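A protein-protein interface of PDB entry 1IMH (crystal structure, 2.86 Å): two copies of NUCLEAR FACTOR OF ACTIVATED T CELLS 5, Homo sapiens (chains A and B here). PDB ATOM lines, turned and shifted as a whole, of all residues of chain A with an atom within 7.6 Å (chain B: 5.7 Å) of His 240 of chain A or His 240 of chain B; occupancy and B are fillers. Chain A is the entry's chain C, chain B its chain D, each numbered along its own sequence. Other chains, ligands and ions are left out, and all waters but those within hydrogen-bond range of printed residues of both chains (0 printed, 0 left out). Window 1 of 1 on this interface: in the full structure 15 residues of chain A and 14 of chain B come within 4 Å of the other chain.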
ATOM      1  N   GLU A 183       0.816  20.665   9.213  1.00  0.00           N
ATOM      2  CA  GLU A 183      -0.265  19.819   8.749  1.00  0.00           C
ATOM      3  C   GLU A 183      -0.108  18.365   9.199  1.00  0.00           C
ATOM      4  O   GLU A 183       0.989  17.800   9.159  1.00  0.00           O
ATOM      5  CB  GLU A 183      -0.341  19.918   7.217  1.00  0.00           C
ATOM      6  CG  GLU A 183      -1.304  18.960   6.546  1.00  0.00           C
ATOM      7  CD  GLU A 183      -1.548  19.300   5.078  1.00  0.00           C
ATOM      8  OE1 GLU A 183      -0.564  19.472   4.320  1.00  0.00           O
ATOM      9  OE2 GLU A 183      -2.733  19.390   4.682  1.00  0.00           O
ATOM     10  N   LEU A 185      -1.222  14.643   8.405  1.00  0.00           N
ATOM     11  CA  LEU A 185      -1.796  13.830   7.340  1.00  0.00           C
ATOM     12  C   LEU A 185      -2.375  12.515   7.842  1.00  0.00           C
ATOM     13  O   LEU A 185      -3.328  12.000   7.268  1.00  0.00           O
ATOM     14  CB  LEU A 185      -0.744  13.545   6.267  1.00  0.00           C
ATOM     15  CG  LEU A 185      -0.132  14.763   5.574  1.00  0.00           C
ATOM     16  CD1 LEU A 185       1.043  14.339   4.704  1.00  0.00           C
ATOM     17  CD2 LEU A 185      -1.202  15.461   4.765  1.00  0.00           C
ATOM     18  N   PHE A 201       1.728   8.150  16.600  1.00  0.00           N
ATOM     19  CA  PHE A 201       2.609   8.587  15.529  1.00  0.00           C
ATOM     20  C   PHE A 201       1.872   9.557  14.620  1.00  0.00           C
ATOM     21  O   PHE A 201       0.785   9.256  14.133  1.00  0.00           O
ATOM     22  CB  PHE A 201       3.090   7.411  14.687  1.00  0.00           C
ATOM     23  CG  PHE A 201       4.111   6.559  15.359  1.00  0.00           C
ATOM     24  CD1 PHE A 201       5.048   5.873  14.608  1.00  0.00           C
ATOM     25  CD2 PHE A 201       4.122   6.421  16.737  1.00  0.00           C
ATOM     26  CE1 PHE A 201       5.977   5.049  15.208  1.00  0.00           C
ATOM     27  CE2 PHE A 201       5.046   5.599  17.354  1.00  0.00           C
ATOM     28  CZ  PHE A 201       5.981   4.911  16.587  1.00  0.00           C
ATOM     29  N   LEU A 202       2.468  10.723  14.399  1.00  0.00           N
ATOM     30  CA  LEU A 202       1.877  11.725  13.529  1.00  0.00           C
ATOM     31  C   LEU A 202       2.763  11.946  12.320  1.00  0.00           C
ATOM     32  O   LEU A 202       3.949  12.258  12.457  1.00  0.00           O
ATOM     33  CB  LEU A 202       1.734  13.054  14.253  1.00  0.00           C
ATOM     34  CG  LEU A 202       0.960  13.084  15.557  1.00  0.00           C
ATOM     35  CD1 LEU A 202       0.793  14.541  16.015  1.00  0.00           C
ATOM     36  CD2 LEU A 202      -0.393  12.417  15.355  1.00  0.00           C
ATOM     37  N   ILE A 203       2.216  11.760  11.131  1.00  0.00           N
ATOM     38  CA  ILE A 203       3.006  12.032   9.948  1.00  0.00           C
ATOM     39  C   ILE A 203       2.255  13.122   9.185  1.00  0.00           C
ATOM     40  O   ILE A 203       1.038  13.064   8.991  1.00  0.00           O
ATOM     41  CB  ILE A 203       3.250  10.758   9.070  1.00  0.00           C
ATOM     42  CG1 ILE A 203       2.031  10.437   8.218  1.00  0.00           C
ATOM     43  CG2 ILE A 203       3.614   9.583   9.945  1.00  0.00           C
ATOM     44  CD1 ILE A 203       2.015  11.182   6.891  1.00  0.00           C
ATOM     45  N   GLY A 204       3.000  14.148   8.807  1.00  0.00           N
ATOM     46  CA  GLY A 204       2.437  15.268   8.083  1.00  0.00           C
ATOM     47  C   GLY A 204       3.586  16.076   7.520  1.00  0.00           C
ATOM     48  O   GLY A 204       4.498  15.527   6.904  1.00  0.00           O
ATOM     49  N   LYS A 205       3.572  17.379   7.749  1.00  0.00           N
ATOM     50  CA  LYS A 205       4.638  18.200   7.218  1.00  0.00           C
ATOM     51  C   LYS A 205       4.783  19.541   7.915  1.00  0.00           C
ATOM     52  O   LYS A 205       3.841  20.061   8.504  1.00  0.00           O
ATOM     53  CB  LYS A 205       4.408  18.419   5.724  1.00  0.00           C
ATOM     54  CG  LYS A 205       3.058  19.026   5.413  1.00  0.00           C
ATOM     55  CD  LYS A 205       2.836  19.194   3.918  1.00  0.00           C
ATOM     56  CE  LYS A 205       2.708  17.850   3.209  1.00  0.00           C
ATOM     57  NZ  LYS A 205       2.346  18.016   1.767  1.00  0.00           N
ATOM     58  N   ASN A 206       5.993  20.083   7.839  1.00  0.00           N
ATOM     59  CA  ASN A 206       6.322  21.377   8.417  1.00  0.00           C
ATOM     60  C   ASN A 206       6.245  21.459   9.926  1.00  0.00           C
ATOM     61  O   ASN A 206       5.662  22.388  10.479  1.00  0.00           O
ATOM     62  CB  ASN A 206       5.443  22.462   7.799  1.00  0.00           C
ATOM     63  CG  ASN A 206       5.674  22.615   6.313  1.00  0.00           C
ATOM     64  OD1 ASN A 206       5.020  23.424   5.662  1.00  0.00           O
ATOM     65  ND2 ASN A 206       6.607  21.841   5.768  1.00  0.00           N
ATOM     66  N   PHE A 207       6.833  20.474  10.587  1.00  0.00           N
ATOM     67  CA  PHE A 207       6.880  20.463  12.040  1.00  0.00           C
ATOM     68  C   PHE A 207       8.206  21.129  12.384  1.00  0.00           C
ATOM     69  O   PHE A 207       9.262  20.474  12.467  1.00  0.00           O
ATOM     70  CB  PHE A 207       6.833  19.030  12.587  1.00  0.00           C
ATOM     71  CG  PHE A 207       5.592  18.273  12.181  1.00  0.00           C
ATOM     72  CD1 PHE A 207       4.380  18.944  12.002  1.00  0.00           C
ATOM     73  CD2 PHE A 207       5.632  16.903  11.970  1.00  0.00           C
ATOM     74  CE1 PHE A 207       3.239  18.261  11.619  1.00  0.00           C
ATOM     75  CE2 PHE A 207       4.493  16.213  11.588  1.00  0.00           C
ATOM     76  CZ  PHE A 207       3.298  16.890  11.409  1.00  0.00           C
ATOM     77  N   ILE A 231       6.222  15.598  23.368  1.00  0.00           N
ATOM     78  CA  ILE A 231       6.814  15.135  22.123  1.00  0.00           C
ATOM     79  C   ILE A 231       8.128  14.433  22.385  1.00  0.00           C
ATOM     80  O   ILE A 231       8.871  14.814  23.276  1.00  0.00           O
ATOM     81  CB  ILE A 231       7.107  16.294  21.144  1.00  0.00           C
ATOM     82  CG1 ILE A 231       5.810  16.990  20.732  1.00  0.00           C
ATOM     83  CG2 ILE A 231       7.799  15.747  19.901  1.00  0.00           C
ATOM     84  CD1 ILE A 231       6.027  18.135  19.778  1.00  0.00           C
ATOM     85  N   ASP A 232       8.403  13.400  21.600  1.00  0.00           N
ATOM     86  CA  ASP A 232       9.647  12.665  21.719  1.00  0.00           C
ATOM     87  C   ASP A 232      10.667  13.442  20.902  1.00  0.00           C
ATOM     88  O   ASP A 232      10.502  13.604  19.695  1.00  0.00           O
ATOM     89  CB  ASP A 232       9.482  11.255  21.150  1.00  0.00           C
ATOM     90  CG  ASP A 232      10.781  10.482  21.133  1.00  0.00           C
ATOM     91  OD1 ASP A 232      10.762   9.279  20.794  1.00  0.00           O
ATOM     92  OD2 ASP A 232      11.829  11.078  21.456  1.00  0.00           O
ATOM     93  N   LEU A 235      13.441  11.746  18.209  1.00  0.00           N
ATOM     94  CA  LEU A 235      12.961  11.327  16.899  1.00  0.00           C
ATOM     95  C   LEU A 235      12.138  12.402  16.249  1.00  0.00           C
ATOM     96  O   LEU A 235      11.276  12.125  15.420  1.00  0.00           O
ATOM     97  CB  LEU A 235      12.131  10.049  17.005  1.00  0.00           C
ATOM     98  CG  LEU A 235      12.923   8.785  17.366  1.00  0.00           C
ATOM     99  CD1 LEU A 235      11.970   7.611  17.544  1.00  0.00           C
ATOM    100  CD2 LEU A 235      13.945   8.486  16.273  1.00  0.00           C
ATOM    101  N   PHE A 236      12.397  13.644  16.626  1.00  0.00           N
ATOM    102  CA  PHE A 236      11.665  14.744  16.035  1.00  0.00           C
ATOM    103  C   PHE A 236      12.021  14.806  14.547  1.00  0.00           C
ATOM    104  O   PHE A 236      13.127  14.437  14.141  1.00  0.00           O
ATOM    105  CB  PHE A 236      12.045  16.048  16.728  1.00  0.00           C
ATOM    106  CG  PHE A 236      11.194  17.208  16.336  1.00  0.00           C
ATOM    107  CD1 PHE A 236      11.189  17.675  15.030  1.00  0.00           C
ATOM    108  CD2 PHE A 236      10.369  17.821  17.271  1.00  0.00           C
ATOM    109  CE1 PHE A 236      10.370  18.741  14.648  1.00  0.00           C
ATOM    110  CE2 PHE A 236       9.540  18.891  16.907  1.00  0.00           C
ATOM    111  CZ  PHE A 236       9.539  19.354  15.587  1.00  0.00           C
ATOM    112  N   HIS A 237      11.070  15.240  13.731  1.00  0.00           N
ATOM    113  CA  HIS A 237      11.295  15.377  12.300  1.00  0.00           C
ATOM    114  C   HIS A 237      10.264  16.324  11.706  1.00  0.00           C
ATOM    115  O   HIS A 237       9.111  16.352  12.132  1.00  0.00           O
ATOM    116  CB  HIS A 237      11.214  14.027  11.594  1.00  0.00           C
ATOM    117  CG  HIS A 237      11.554  14.099  10.139  1.00  0.00           C
ATOM    118  ND1 HIS A 237      10.774  14.776   9.227  1.00  0.00           N
ATOM    119  CD2 HIS A 237      12.614  13.619   9.446  1.00  0.00           C
ATOM    120  CE1 HIS A 237      11.339  14.709   8.033  1.00  0.00           C
ATOM    121  NE2 HIS A 237      12.456  14.012   8.140  1.00  0.00           N
ATOM    122  N   GLN A 238      10.682  17.099  10.715  1.00  0.00           N
ATOM    123  CA  GLN A 238       9.791  18.050  10.092  1.00  0.00           C
ATOM    124  C   GLN A 238       8.528  17.405   9.527  1.00  0.00           C
ATOM    125  O   GLN A 238       7.479  18.049   9.445  1.00  0.00           O
ATOM    126  CB  GLN A 238      10.531  18.790   8.982  1.00  0.00           C
ATOM    127  CG  GLN A 238       9.676  19.812   8.267  1.00  0.00           C
ATOM    128  CD  GLN A 238      10.405  20.468   7.131  1.00  0.00           C
ATOM    129  OE1 GLN A 238      11.416  21.143   7.336  1.00  0.00           O
ATOM    130  NE2 GLN A 238       9.903  20.271   5.917  1.00  0.00           N
ATOM    131  N   ASN A 239       8.619  16.134   9.149  1.00  0.00           N
ATOM    132  CA  ASN A 239       7.468  15.444   8.567  1.00  0.00           C
ATOM    133  C   ASN A 239       6.759  14.438   9.452  1.00  0.00           C
ATOM    134  O   ASN A 239       5.672  13.987   9.113  1.00  0.00           O
ATOM    135  CB  ASN A 239       7.876  14.768   7.261  1.00  0.00           C
ATOM    136  CG  ASN A 239       8.141  15.765   6.155  1.00  0.00           C
ATOM    137  OD1 ASN A 239       7.221  16.411   5.656  1.00  0.00           O
ATOM    138  ND2 ASN A 239       9.404  15.905   5.774  1.00  0.00           N
ATOM    139  N   HIS A 240       7.361  14.075  10.578  1.00  0.00           N
ATOM    140  CA  HIS A 240       6.720  13.122  11.470  1.00  0.00           C
ATOM    141  C   HIS A 240       7.141  13.364  12.903  1.00  0.00           C
ATOM    142  O   HIS A 240       8.193  13.947  13.145  1.00  0.00           O
ATOM    143  CB  HIS A 240       7.068  11.691  11.047  1.00  0.00           C
ATOM    144  CG  HIS A 240       8.498  11.311  11.272  1.00  0.00           C
ATOM    145  ND1 HIS A 240       9.282  10.749  10.287  1.00  0.00           N
ATOM    146  CD2 HIS A 240       9.269  11.347  12.387  1.00  0.00           C
ATOM    147  CE1 HIS A 240      10.471  10.454  10.783  1.00  0.00           C
ATOM    148  NE2 HIS A 240      10.490  10.805  12.057  1.00  0.00           N
ATOM    149  N   LEU A 241       6.320  12.937  13.856  1.00  0.00           N
ATOM    150  CA  LEU A 241       6.664  13.102  15.263  1.00  0.00           C
ATOM    151  C   LEU A 241       5.860  12.184  16.188  1.00  0.00           C
ATOM    152  O   LEU A 241       4.693  11.888  15.939  1.00  0.00           O
ATOM    153  CB  LEU A 241       6.526  14.580  15.668  1.00  0.00           C
ATOM    154  CG  LEU A 241       5.191  15.292  15.497  1.00  0.00           C
ATOM    155  CD1 LEU A 241       4.265  14.814  16.614  1.00  0.00           C
ATOM    156  CD2 LEU A 241       5.353  16.818  15.556  1.00  0.00           C
ATOM    157  N   ILE A 242       6.501  11.714  17.250  1.00  0.00           N
ATOM    158  CA  ILE A 242       5.845  10.816  18.198  1.00  0.00           C
ATOM    159  C   ILE A 242       5.499  11.504  19.513  1.00  0.00           C
ATOM    160  O   ILE A 242       6.384  11.933  20.249  1.00  0.00           O
ATOM    161  CB  ILE A 242       6.741   9.601  18.492  1.00  0.00           C
ATOM    162  CG1 ILE A 242       7.019   8.849  17.190  1.00  0.00           C
ATOM    163  CG2 ILE A 242       6.073   8.688  19.504  1.00  0.00           C
ATOM    164  CD1 ILE A 242       8.065   7.789  17.321  1.00  0.00           C
ATOM    165  N   LEU B 202       6.200   3.087  10.690  1.00  0.00           N
ATOM    166  CA  LEU B 202       7.610   2.819  10.880  1.00  0.00           C
ATOM    167  C   LEU B 202       8.411   4.094  10.676  1.00  0.00           C
ATOM    168  O   LEU B 202       8.318   4.730   9.619  1.00  0.00           O
ATOM    169  CB  LEU B 202       8.106   1.783   9.876  1.00  0.00           C
ATOM    170  CG  LEU B 202       7.413   0.428   9.805  1.00  0.00           C
ATOM    171  CD1 LEU B 202       8.189  -0.487   8.857  1.00  0.00           C
ATOM    172  CD2 LEU B 202       7.333  -0.173  11.195  1.00  0.00           C
ATOM    173  N   ILE B 203       9.177   4.495  11.684  1.00  0.00           N
ATOM    174  CA  ILE B 203      10.008   5.662  11.508  1.00  0.00           C
ATOM    175  C   ILE B 203      11.447   5.187  11.705  1.00  0.00           C
ATOM    176  O   ILE B 203      11.770   4.464  12.659  1.00  0.00           O
ATOM    177  CB  ILE B 203       9.632   6.827  12.479  1.00  0.00           C
ATOM    178  CG1 ILE B 203      10.214   6.595  13.865  1.00  0.00           C
ATOM    179  CG2 ILE B 203       8.133   6.981  12.548  1.00  0.00           C
ATOM    180  CD1 ILE B 203      11.641   7.100  14.018  1.00  0.00           C
ATOM    181  N   GLY B 204      12.292   5.561  10.754  1.00  0.00           N
ATOM    182  CA  GLY B 204      13.688   5.185  10.788  1.00  0.00           C
ATOM    183  C   GLY B 204      14.419   6.046   9.783  1.00  0.00           C
ATOM    184  O   GLY B 204      14.256   7.266   9.773  1.00  0.00           O
ATOM    185  N   PHE B 207      14.893   4.906   3.625  1.00  0.00           N
ATOM    186  CA  PHE B 207      13.911   4.069   2.967  1.00  0.00           C
ATOM    187  C   PHE B 207      13.905   4.551   1.525  1.00  0.00           C
ATOM    188  O   PHE B 207      13.165   5.469   1.150  1.00  0.00           O
ATOM    189  CB  PHE B 207      12.529   4.229   3.612  1.00  0.00           C
ATOM    190  CG  PHE B 207      12.497   3.868   5.075  1.00  0.00           C
ATOM    191  CD1 PHE B 207      13.326   2.864   5.577  1.00  0.00           C
ATOM    192  CD2 PHE B 207      11.644   4.525   5.952  1.00  0.00           C
ATOM    193  CE1 PHE B 207      13.312   2.526   6.930  1.00  0.00           C
ATOM    194  CE2 PHE B 207      11.626   4.192   7.303  1.00  0.00           C
ATOM    195  CZ  PHE B 207      12.462   3.188   7.791  1.00  0.00           C
ATOM    196  N   LEU B 235       2.243   8.207   0.992  1.00  0.00           N
ATOM    197  CA  LEU B 235       2.909   8.809   2.146  1.00  0.00           C
ATOM    198  C   LEU B 235       4.285   8.220   2.347  1.00  0.00           C
ATOM    199  O   LEU B 235       4.818   8.208   3.455  1.00  0.00           O
ATOM    200  CB  LEU B 235       2.082   8.620   3.422  1.00  0.00           C
ATOM    201  CG  LEU B 235       0.785   9.433   3.481  1.00  0.00           C
ATOM    202  CD1 LEU B 235       0.014   9.083   4.740  1.00  0.00           C
ATOM    203  CD2 LEU B 235       1.107  10.919   3.438  1.00  0.00           C
ATOM    204  N   PHE B 236       4.869   7.726   1.270  1.00  0.00           N
ATOM    205  CA  PHE B 236       6.196   7.159   1.370  1.00  0.00           C
ATOM    206  C   PHE B 236       7.165   8.284   1.741  1.00  0.00           C
ATOM    207  O   PHE B 236       6.958   9.441   1.380  1.00  0.00           O
ATOM    208  CB  PHE B 236       6.591   6.531   0.032  1.00  0.00           C
ATOM    209  CG  PHE B 236       7.854   5.734   0.092  1.00  0.00           C
ATOM    210  CD1 PHE B 236       9.066   6.347   0.387  1.00  0.00           C
ATOM    211  CD2 PHE B 236       7.832   4.364  -0.128  1.00  0.00           C
ATOM    212  CE1 PHE B 236      10.243   5.609   0.470  1.00  0.00           C
ATOM    213  CE2 PHE B 236       9.004   3.609  -0.049  1.00  0.00           C
ATOM    214  CZ  PHE B 236      10.214   4.233   0.249  1.00  0.00           C
ATOM    215  N   HIS B 237       8.213   7.941   2.479  1.00  0.00           N
ATOM    216  CA  HIS B 237       9.220   8.915   2.876  1.00  0.00           C
ATOM    217  C   HIS B 237      10.493   8.188   3.272  1.00  0.00           C
ATOM    218  O   HIS B 237      10.453   7.098   3.844  1.00  0.00           O
ATOM    219  CB  HIS B 237       8.737   9.766   4.048  1.00  0.00           C
ATOM    220  CG  HIS B 237       9.688  10.859   4.423  1.00  0.00           C
ATOM    221  ND1 HIS B 237      10.933  10.609   4.965  1.00  0.00           N
ATOM    222  CD2 HIS B 237       9.599  12.205   4.290  1.00  0.00           C
ATOM    223  CE1 HIS B 237      11.569  11.754   5.147  1.00  0.00           C
ATOM    224  NE2 HIS B 237      10.780  12.737   4.746  1.00  0.00           N
ATOM    225  N   GLN B 238      11.629   8.796   2.968  1.00  0.00           N
ATOM    226  CA  GLN B 238      12.902   8.190   3.285  1.00  0.00           C
ATOM    227  C   GLN B 238      13.059   7.866   4.769  1.00  0.00           C
ATOM    228  O   GLN B 238      13.776   6.933   5.131  1.00  0.00           O
ATOM    229  CB  GLN B 238      14.031   9.113   2.840  1.00  0.00           C
ATOM    230  CG  GLN B 238      15.412   8.564   3.124  1.00  0.00           C
ATOM    231  CD  GLN B 238      16.502   9.529   2.739  1.00  0.00           C
ATOM    232  OE1 GLN B 238      16.655   9.877   1.570  1.00  0.00           O
ATOM    233  NE2 GLN B 238      17.267   9.970   3.725  1.00  0.00           N
ATOM    234  N   ASN B 239      12.387   8.624   5.629  1.00  0.00           N
ATOM    235  CA  ASN B 239      12.509   8.404   7.064  1.00  0.00           C
ATOM    236  C   ASN B 239      11.330   7.741   7.749  1.00  0.00           C
ATOM    237  O   ASN B 239      11.436   7.339   8.899  1.00  0.00           O
ATOM    238  CB  ASN B 239      12.823   9.722   7.763  1.00  0.00           C
ATOM    239  CG  ASN B 239      14.222  10.209   7.466  1.00  0.00           C
ATOM    240  OD1 ASN B 239      15.205   9.620   7.914  1.00  0.00           O
ATOM    241  ND2 ASN B 239      14.321  11.285   6.696  1.00  0.00           N
ATOM    242  N   HIS B 240      10.205   7.621   7.062  1.00  0.00           N
ATOM    243  CA  HIS B 240       9.057   6.981   7.678  1.00  0.00           C
ATOM    244  C   HIS B 240       8.183   6.328   6.616  1.00  0.00           C
ATOM    245  O   HIS B 240       8.225   6.719   5.452  1.00  0.00           O
ATOM    246  CB  HIS B 240       8.245   8.014   8.476  1.00  0.00           C
ATOM    247  CG  HIS B 240       7.529   9.031   7.629  1.00  0.00           C
ATOM    248  ND1 HIS B 240       7.623  10.386   7.861  1.00  0.00           N
ATOM    249  CD2 HIS B 240       6.654   8.888   6.600  1.00  0.00           C
ATOM    250  CE1 HIS B 240       6.838  11.035   7.017  1.00  0.00           C
ATOM    251  NE2 HIS B 240       6.239  10.150   6.241  1.00  0.00           N
ATOM    252  N   LEU B 241       7.397   5.329   7.009  1.00  0.00           N
ATOM    253  CA  LEU B 241       6.501   4.665   6.062  1.00  0.00           C
ATOM    254  C   LEU B 241       5.387   3.877   6.748  1.00  0.00           C
ATOM    255  O   LEU B 241       5.572   3.315   7.817  1.00  0.00           O
ATOM    256  CB  LEU B 241       7.313   3.777   5.105  1.00  0.00           C
ATOM    257  CG  LEU B 241       8.206   2.671   5.664  1.00  0.00           C
ATOM    258  CD1 LEU B 241       7.317   1.517   6.079  1.00  0.00           C
ATOM    259  CD2 LEU B 241       9.222   2.209   4.620  1.00  0.00           C
ATOM    260  N   ILE B 242       4.216   3.863   6.133  1.00  0.00           N
ATOM    261  CA  ILE B 242       3.068   3.156   6.691  1.00  0.00           C
ATOM    262  C   ILE B 242       2.751   1.868   5.932  1.00  0.00           C
ATOM    263  O   ILE B 242       2.404   1.897   4.753  1.00  0.00           O
ATOM    264  CB  ILE B 242       1.827   4.059   6.677  1.00  0.00           C
ATOM    265  CG1 ILE B 242       2.105   5.315   7.510  1.00  0.00           C
ATOM    266  CG2 ILE B 242       0.628   3.303   7.209  1.00  0.00           C
ATOM    267  CD1 ILE B 242       1.048   6.379   7.383  1.00  0.00           C
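Of chain B, only Asn 239 and His 240 come within 4 Å of His 240 of chain A.
His 240 of chain B touches just these residues of chain A: Asn 239 and His 240.
Printed residues of chain B within 4 Å of Ile 203 of chain A: Leu 235.
Of the printed residues of chain B, Asn 239 of chain A touches His 237 and His 240.
Of the printed residues of chain B, Leu 235 of chain A touches Ile 203 (3.5 Å).
The nearest residue of chain B that does not touch His 240 of chain A is Ile 203 of chain B (4.1 Å).
The nearest residue of chain A that does not touch His 240 of chain B is Ile 203 of chain A (4.1 Å).
The backbone NH (N) of Leu 185 of chain A sits at hydrogen-bond distance from the backbone carbonyl oxygen (O) of Ile 203 of chain A (2.8 Å).
A ring nitrogen (ND1) of His 237 of chain B lies within hydrogen-bond range of the backbone NH of Asn 239 of chain B, at 2.5 Å.
O of Asn 239 of chain B is in hydrogen-bond range of N of Gly 204 of chain B, 2.7 Å away.
A ring nitrogen (ND1) of His 237 of chain A lies within hydrogen-bond range of the backbone NH of Asn 239 of chain A, 2.5 Å away.
O of Asn 239 of chain A lies within hydrogen-bond range of N of Gly 204 of chain A.
A ring nitrogen (ND1) of His 240 of chain A lies within hydrogen-bond range of a ring nitrogen (ND1) of His 240 of chain B (3.0 Å).
Ile 203 of chain A touches Leu 235 of chain B, and with the chains exchanged Leu 235 of chain A touches Ile 203 of chain B.
His 237 of chain B touches its own counterpart, His 237 of chain A.
His 237 of chain A touches Asn 239 of chain B, and with the chains exchanged Asn 239 of chain A touches His 237 of chain B.
Asn 239 of chain A touches His 240 of chain B, and with the chains exchanged His 240 of chain A touches Asn 239 of chain B.
Positions printed for both chains: 202, 203, 204, 207, 235, 236, 237, 238, 239, 240, 241 and 242.
Of the 10 pairs that touch across the chains among the printed residues, 8 have their exchanged pair printed and touching as well.
Of the 19 printed residues of chain A, 7 touch a printed residue of chain B.
Printed residues of chain B that touch a printed residue of chain A: Ile 203, Leu 235, His 237, Asn 239 and His 240.
Hydrophobic or aromatic side chains of chain B that line the printed part of chain A: Ile 203, Leu 235, His 237 and His 240.
Among the printed residues, no Asp or Glu carboxylate lies within 4 Å of a Lys or Arg side-chain nitrogen of the other chain.
Among the printed residues, pairs that only touch across the chains: Leu 185 of chain A with Leu 235 of chain B (3.6 Å), Phe 201 of chain A with Ile 203 of chain B (3.9 Å), Ile 203 of chain A with Leu 235 of chain B (3.6 Å), Leu 235 of chain A with Ile 203 of chain B (3.5 Å), His 237 of chain A with His 237 of chain B (3.9 Å), His 237 of chain A with Asn 239 of chain B (3.6 Å), Asn 239 of chain A with His 237 of chain B (3.6 Å), Asn 239 of chain A with His 240 of chain B (3.8 Å) and His 240 of chain A with Asn 239 of chain B (3.8 Å).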
